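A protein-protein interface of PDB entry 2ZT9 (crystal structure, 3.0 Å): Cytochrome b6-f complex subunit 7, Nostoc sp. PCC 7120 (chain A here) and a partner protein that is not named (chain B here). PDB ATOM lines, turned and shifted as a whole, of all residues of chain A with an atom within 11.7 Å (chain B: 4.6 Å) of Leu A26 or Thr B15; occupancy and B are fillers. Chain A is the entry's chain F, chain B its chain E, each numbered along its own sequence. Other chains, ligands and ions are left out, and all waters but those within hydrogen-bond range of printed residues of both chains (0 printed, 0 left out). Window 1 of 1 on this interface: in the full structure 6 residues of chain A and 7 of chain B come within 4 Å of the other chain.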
ATOM      1  N   PHE A  17      13.454  17.591 -11.277  1.00  0.00           N
ATOM      2  CA  PHE A  17      14.057  16.263 -11.082  1.00  0.00           C
ATOM      3  C   PHE A  17      15.362  16.093 -11.852  1.00  0.00           C
ATOM      4  O   PHE A  17      16.303  15.466 -11.352  1.00  0.00           O
ATOM      5  CB  PHE A  17      13.063  15.158 -11.431  1.00  0.00           C
ATOM      6  CG  PHE A  17      11.815  15.209 -10.611  1.00  0.00           C
ATOM      7  CD1 PHE A  17      10.679  15.862 -11.089  1.00  0.00           C
ATOM      8  CD2 PHE A  17      11.776  14.628  -9.342  1.00  0.00           C
ATOM      9  CE1 PHE A  17       9.516  15.924 -10.321  1.00  0.00           C
ATOM     10  CE2 PHE A  17      10.619  14.690  -8.564  1.00  0.00           C
ATOM     11  CZ  PHE A  17       9.487  15.341  -9.053  1.00  0.00           C
ATOM     12  N   VAL A  18      15.425  16.671 -13.053  1.00  0.00           N
ATOM     13  CA  VAL A  18      16.666  16.687 -13.821  1.00  0.00           C
ATOM     14  C   VAL A  18      17.738  17.469 -13.060  1.00  0.00           C
ATOM     15  O   VAL A  18      18.890  17.048 -12.996  1.00  0.00           O
ATOM     16  CB  VAL A  18      16.470  17.287 -15.232  1.00  0.00           C
ATOM     17  CG1 VAL A  18      17.725  17.093 -16.078  1.00  0.00           C
ATOM     18  CG2 VAL A  18      15.253  16.667 -15.919  1.00  0.00           C
ATOM     19  N   GLY A  19      17.344  18.601 -12.476  1.00  0.00           N
ATOM     20  CA  GLY A  19      18.260  19.439 -11.702  1.00  0.00           C
ATOM     21  C   GLY A  19      18.684  18.744 -10.428  1.00  0.00           C
ATOM     22  O   GLY A  19      19.873  18.700 -10.102  1.00  0.00           O
ATOM     23  N   TRP A  20      17.696  18.198  -9.719  1.00  0.00           N
ATOM     24  CA  TRP A  20      17.913  17.384  -8.530  1.00  0.00           C
ATOM     25  C   TRP A  20      18.890  16.230  -8.791  1.00  0.00           C
ATOM     26  O   TRP A  20      19.939  16.144  -8.142  1.00  0.00           O
ATOM     27  CB  TRP A  20      16.573  16.849  -8.033  1.00  0.00           C
ATOM     28  CG  TRP A  20      16.635  16.078  -6.745  1.00  0.00           C
ATOM     29  CD1 TRP A  20      17.698  15.965  -5.889  1.00  0.00           C
ATOM     30  CD2 TRP A  20      15.563  15.339  -6.152  1.00  0.00           C
ATOM     31  NE1 TRP A  20      17.354  15.188  -4.815  1.00  0.00           N
ATOM     32  CE2 TRP A  20      16.049  14.793  -4.947  1.00  0.00           C
ATOM     33  CE3 TRP A  20      14.239  15.079  -6.529  1.00  0.00           C
ATOM     34  CZ2 TRP A  20      15.257  14.002  -4.110  1.00  0.00           C
ATOM     35  CZ3 TRP A  20      13.451  14.291  -5.696  1.00  0.00           C
ATOM     36  CH2 TRP A  20      13.965  13.763  -4.498  1.00  0.00           C
ATOM     37  N   ALA A  21      18.540  15.361  -9.743  1.00  0.00           N
ATOM     38  CA  ALA A  21      19.403  14.253 -10.160  1.00  0.00           C
ATOM     39  C   ALA A  21      20.821  14.727 -10.470  1.00  0.00           C
ATOM     40  O   ALA A  21      21.800  14.114 -10.035  1.00  0.00           O
ATOM     41  CB  ALA A  21      18.809  13.530 -11.370  1.00  0.00           C
ATOM     42  N   LEU A  22      20.919  15.829 -11.208  1.00  0.00           N
ATOM     43  CA  LEU A  22      22.205  16.356 -11.641  1.00  0.00           C
ATOM     44  C   LEU A  22      22.989  16.915 -10.462  1.00  0.00           C
ATOM     45  O   LEU A  22      24.223  16.981 -10.500  1.00  0.00           O
ATOM     46  CB  LEU A  22      21.997  17.441 -12.689  1.00  0.00           C
ATOM     47  CG  LEU A  22      22.809  17.277 -13.972  1.00  0.00           C
ATOM     48  CD1 LEU A  22      22.078  17.949 -15.141  1.00  0.00           C
ATOM     49  CD2 LEU A  22      24.216  17.825 -13.804  1.00  0.00           C
ATOM     50  N   GLY A  23      22.261  17.322  -9.421  1.00  0.00           N
ATOM     51  CA  GLY A  23      22.876  17.820  -8.200  1.00  0.00           C
ATOM     52  C   GLY A  23      23.398  16.643  -7.415  1.00  0.00           C
ATOM     53  O   GLY A  23      24.544  16.653  -6.951  1.00  0.00           O
ATOM     54  N   ALA A  24      22.537  15.628  -7.284  1.00  0.00           N
ATOM     55  CA  ALA A  24      22.872  14.345  -6.657  1.00  0.00           C
ATOM     56  C   ALA A  24      24.104  13.729  -7.317  1.00  0.00           C
ATOM     57  O   ALA A  24      25.046  13.325  -6.626  1.00  0.00           O
ATOM     58  CB  ALA A  24      21.685  13.385  -6.720  1.00  0.00           C
ATOM     59  N   LEU A  25      24.098  13.692  -8.652  1.00  0.00           N
ATOM     60  CA  LEU A  25      25.234  13.193  -9.416  1.00  0.00           C
ATOM     61  C   LEU A  25      26.514  13.883  -8.944  1.00  0.00           C
ATOM     62  O   LEU A  25      27.411  13.227  -8.426  1.00  0.00           O
ATOM     63  CB  LEU A  25      25.028  13.399 -10.925  1.00  0.00           C
ATOM     64  CG  LEU A  25      25.546  12.331 -11.911  1.00  0.00           C
ATOM     65  CD1 LEU A  25      25.527  12.865 -13.340  1.00  0.00           C
ATOM     66  CD2 LEU A  25      26.937  11.791 -11.575  1.00  0.00           C
ATOM     67  N   LEU A  26      26.577  15.204  -9.091  1.00  0.00           N
ATOM     68  CA  LEU A  26      27.762  15.972  -8.712  1.00  0.00           C
ATOM     69  C   LEU A  26      28.236  15.679  -7.292  1.00  0.00           C
ATOM     70  O   LEU A  26      29.439  15.733  -7.020  1.00  0.00           O
ATOM     71  CB  LEU A  26      27.525  17.476  -8.886  1.00  0.00           C
ATOM     72  CG  LEU A  26      27.950  18.168 -10.183  1.00  0.00           C
ATOM     73  CD1 LEU A  26      29.413  17.908 -10.498  1.00  0.00           C
ATOM     74  CD2 LEU A  26      27.084  17.744 -11.337  1.00  0.00           C
ATOM     75  N   LEU A  27      27.294  15.367  -6.397  1.00  0.00           N
ATOM     76  CA  LEU A  27      27.625  15.031  -5.004  1.00  0.00           C
ATOM     77  C   LEU A  27      28.322  13.678  -4.880  1.00  0.00           C
ATOM     78  O   LEU A  27      29.291  13.544  -4.125  1.00  0.00           O
ATOM     79  CB  LEU A  27      26.388  15.085  -4.104  1.00  0.00           C
ATOM     80  CG  LEU A  27      25.995  16.453  -3.541  1.00  0.00           C
ATOM     81  CD1 LEU A  27      24.619  16.368  -2.904  1.00  0.00           C
ATOM     82  CD2 LEU A  27      27.026  16.992  -2.538  1.00  0.00           C
ATOM     83  N   LYS A  28      27.833  12.688  -5.623  1.00  0.00           N
ATOM     84  CA  LYS A  28      28.503  11.389  -5.710  1.00  0.00           C
ATOM     85  C   LYS A  28      29.918  11.526  -6.277  1.00  0.00           C
ATOM     86  O   LYS A  28      30.871  11.023  -5.681  1.00  0.00           O
ATOM     87  CB  LYS A  28      27.693  10.380  -6.535  1.00  0.00           C
ATOM     88  CG  LYS A  28      26.333  10.017  -5.939  1.00  0.00           C
ATOM     89  CD  LYS A  28      26.184   8.509  -5.778  1.00  0.00           C
ATOM     90  CE  LYS A  28      26.821   8.034  -4.465  1.00  0.00           C
ATOM     91  NZ  LYS A  28      27.147   6.579  -4.481  1.00  0.00           N
ATOM     92  N   ILE A  29      30.055  12.225  -7.406  1.00  0.00           N
ATOM     93  CA  ILE A  29      31.362  12.380  -8.065  1.00  0.00           C
ATOM     94  C   ILE A  29      32.377  13.212  -7.261  1.00  0.00           C
ATOM     95  O   ILE A  29      33.557  13.271  -7.617  1.00  0.00           O
ATOM     96  CB  ILE A  29      31.247  12.822  -9.582  1.00  0.00           C
ATOM     97  CG1 ILE A  29      32.340  13.823  -9.979  1.00  0.00           C
ATOM     98  CG2 ILE A  29      29.881  13.392  -9.905  1.00  0.00           C
ATOM     99  CD1 ILE A  29      32.239  14.287 -11.415  1.00  0.00           C
ATOM    100  N   GLN A  30      31.926  13.828  -6.171  1.00  0.00           N
ATOM    101  CA  GLN A  30      32.841  14.578  -5.312  1.00  0.00           C
ATOM    102  C   GLN A  30      33.243  13.775  -4.078  1.00  0.00           C
ATOM    103  O   GLN A  30      34.289  14.032  -3.480  1.00  0.00           O
ATOM    104  CB  GLN A  30      32.270  15.955  -4.927  1.00  0.00           C
ATOM    105  CG  GLN A  30      31.400  15.989  -3.671  1.00  0.00           C
ATOM    106  CD  GLN A  30      31.671  17.200  -2.787  1.00  0.00           C
ATOM    107  OE1 GLN A  30      30.849  17.575  -1.954  1.00  0.00           O
ATOM    108  NE2 GLN A  30      32.828  17.809  -2.963  1.00  0.00           N
ATOM    109  N   GLY A  31      32.412  12.803  -3.709  1.00  0.00           N
ATOM    110  CA  GLY A  31      32.648  11.996  -2.515  1.00  0.00           C
ATOM    111  C   GLY A  31      32.082  12.628  -1.254  1.00  0.00           C
ATOM    112  O   GLY A  31      32.837  13.020  -0.355  1.00  0.00           O
ATOM    113  N   ALA A  32      30.749  12.713  -1.190  1.00  0.00           N
ATOM    114  CA  ALA A  32      30.027  13.340  -0.076  1.00  0.00           C
ATOM    115  C   ALA A  32      30.180  12.568   1.233  1.00  0.00           C
ATOM    116  O   ALA A  32      30.193  13.159   2.316  1.00  0.00           O
ATOM    117  CB  ALA A  32      28.546  13.498  -0.427  1.00  0.00           C
ATOM    118  N   LEU B  11      23.975  21.118 -20.674  1.00  0.00           N
ATOM    119  CA  LEU B  11      24.141  20.573 -19.329  1.00  0.00           C
ATOM    120  C   LEU B  11      25.354  19.647 -19.217  1.00  0.00           C
ATOM    121  O   LEU B  11      26.112  19.741 -18.251  1.00  0.00           O
ATOM    122  CB  LEU B  11      22.863  19.879 -18.853  1.00  0.00           C
ATOM    123  CG  LEU B  11      21.678  20.791 -18.507  1.00  0.00           C
ATOM    124  CD1 LEU B  11      20.442  19.963 -18.239  1.00  0.00           C
ATOM    125  CD2 LEU B  11      21.968  21.703 -17.315  1.00  0.00           C
ATOM    126  N   ALA B  12      25.536  18.768 -20.205  1.00  0.00           N
ATOM    127  CA  ALA B  12      26.740  17.940 -20.297  1.00  0.00           C
ATOM    128  C   ALA B  12      27.990  18.814 -20.244  1.00  0.00           C
ATOM    129  O   ALA B  12      28.845  18.622 -19.376  1.00  0.00           O
ATOM    130  CB  ALA B  12      26.731  17.110 -21.565  1.00  0.00           C
ATOM    131  N   LEU B  13      28.081  19.786 -21.153  1.00  0.00           N
ATOM    132  CA  LEU B  13      29.221  20.696 -21.186  1.00  0.00           C
ATOM    133  C   LEU B  13      29.497  21.333 -19.819  1.00  0.00           C
ATOM    134  O   LEU B  13      30.648  21.401 -19.391  1.00  0.00           O
ATOM    135  CB  LEU B  13      29.037  21.773 -22.267  1.00  0.00           C
ATOM    136  CG  LEU B  13      29.938  23.017 -22.172  1.00  0.00           C
ATOM    137  CD1 LEU B  13      31.411  22.689 -22.461  1.00  0.00           C
ATOM    138  CD2 LEU B  13      29.444  24.147 -23.067  1.00  0.00           C
ATOM    139  N   PHE B  14      28.446  21.790 -19.138  1.00  0.00           N
ATOM    140  CA  PHE B  14      28.615  22.465 -17.849  1.00  0.00           C
ATOM    141  C   PHE B  14      28.865  21.523 -16.668  1.00  0.00           C
ATOM    142  O   PHE B  14      29.586  21.879 -15.734  1.00  0.00           O
ATOM    143  CB  PHE B  14      27.470  23.451 -17.567  1.00  0.00           C
ATOM    144  CG  PHE B  14      27.793  24.876 -17.958  1.00  0.00           C
ATOM    145  CD1 PHE B  14      27.485  25.355 -19.227  1.00  0.00           C
ATOM    146  CD2 PHE B  14      28.433  25.729 -17.059  1.00  0.00           C
ATOM    147  CE1 PHE B  14      27.799  26.669 -19.588  1.00  0.00           C
ATOM    148  CE2 PHE B  14      28.753  27.041 -17.417  1.00  0.00           C
ATOM    149  CZ  PHE B  14      28.434  27.510 -18.681  1.00  0.00           C
ATOM    150  N   THR B  15      28.289  20.323 -16.717  1.00  0.00           N
ATOM    151  CA  THR B  15      28.679  19.255 -15.787  1.00  0.00           C
ATOM    152  C   THR B  15      30.151  18.915 -16.033  1.00  0.00           C
ATOM    153  O   THR B  15      30.920  18.706 -15.088  1.00  0.00           O
ATOM    154  CB  THR B  15      27.805  17.994 -15.943  1.00  0.00           C
ATOM    155  OG1 THR B  15      26.421  18.358 -15.871  1.00  0.00           O
ATOM    156  CG2 THR B  15      28.109  16.985 -14.848  1.00  0.00           C
ATOM    157  N   GLY B  16      30.529  18.884 -17.312  1.00  0.00           N
ATOM    158  CA  GLY B  16      31.921  18.768 -17.711  1.00  0.00           C
ATOM    159  C   GLY B  16      32.775  19.785 -16.982  1.00  0.00           C
ATOM    160  O   GLY B  16      33.698  19.416 -16.263  1.00  0.00           O
ATOM    161  N   ILE B  17      32.441  21.066 -17.141  1.00  0.00           N
ATOM    162  CA  ILE B  17      33.209  22.156 -16.534  1.00  0.00           C
ATOM    163  C   ILE B  17      33.184  22.080 -15.001  1.00  0.00           C
ATOM    164  O   ILE B  17      34.181  22.388 -14.349  1.00  0.00           O
ATOM    165  CB  ILE B  17      32.753  23.557 -17.051  1.00  0.00           C
ATOM    166  CG1 ILE B  17      32.893  23.640 -18.579  1.00  0.00           C
ATOM    167  CG2 ILE B  17      33.571  24.678 -16.408  1.00  0.00           C
ATOM    168  CD1 ILE B  17      32.131  24.792 -19.231  1.00  0.00           C
ATOM    169  N   ALA B  18      32.057  21.650 -14.434  1.00  0.00           N
ATOM    170  CA  ALA B  18      31.946  21.472 -12.983  1.00  0.00           C
ATOM    171  C   ALA B  18      32.957  20.440 -12.487  1.00  0.00           C
ATOM    172  O   ALA B  18      33.806  20.749 -11.641  1.00  0.00           O
ATOM    173  CB  ALA B  18      30.535  21.067 -12.593  1.00  0.00           C
ATOM    174  N   ALA B  19      32.867  19.225 -13.037  1.00  0.00           N
ATOM    175  CA  ALA B  19      33.798  18.137 -12.728  1.00  0.00           C
ATOM    176  C   ALA B  19      35.231  18.558 -13.029  1.00  0.00           C
ATOM    177  O   ALA B  19      36.065  18.613 -12.125  1.00  0.00           O
ATOM    178  CB  ALA B  19      33.434  16.898 -13.510  1.00  0.00           C
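Among the printed residues, merely in contact across the chains: Leu A22 with Thr B15, Leu A26 with Thr B15, Leu A26 with Ala B18 and Ile A29 with Ala B19.
Of the printed residues of chain B, Leu A22 touches Thr B15.
Leu A26 touches just these residues of chain B: Thr B15 (3.7 Å) and Ala B18 (3.95 Å).
Printed residues of chain B within 4 Å of Ile A29: Ala B19 (3.6 Å).
No residue of chain A comes within 4 Å of Ala B12.
Leu B13 touches none of the printed residues of chain A.
Thr B15 touches just these residues of chain A: Leu A22 (3.1 Å) and Leu A26 (3.7 Å).
No residue of chain A comes within 4 Å of Ile B17.
Of the printed residues of chain A, Ala B19 touches Ile A29 (3.6 Å).
The nearest residue of chain A that does not touch Thr B15 is Leu A25 (5.1 Å).
The nearest printed residue of chain B that does not touch Ile A29 is Thr B15 (5.9 Å).
O of Leu B11 is in hydrogen-bond range of OG1 of Thr B15.
Of the 9 printed residues of chain B, 3 touch a printed residue of chain A.
Among the printed residues, 4 pairs touch across the chains.
Among the printed residues, no Asp or Glu carboxylate lies within 4 Å of a Lys or Arg side-chain nitrogen of the other chain.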
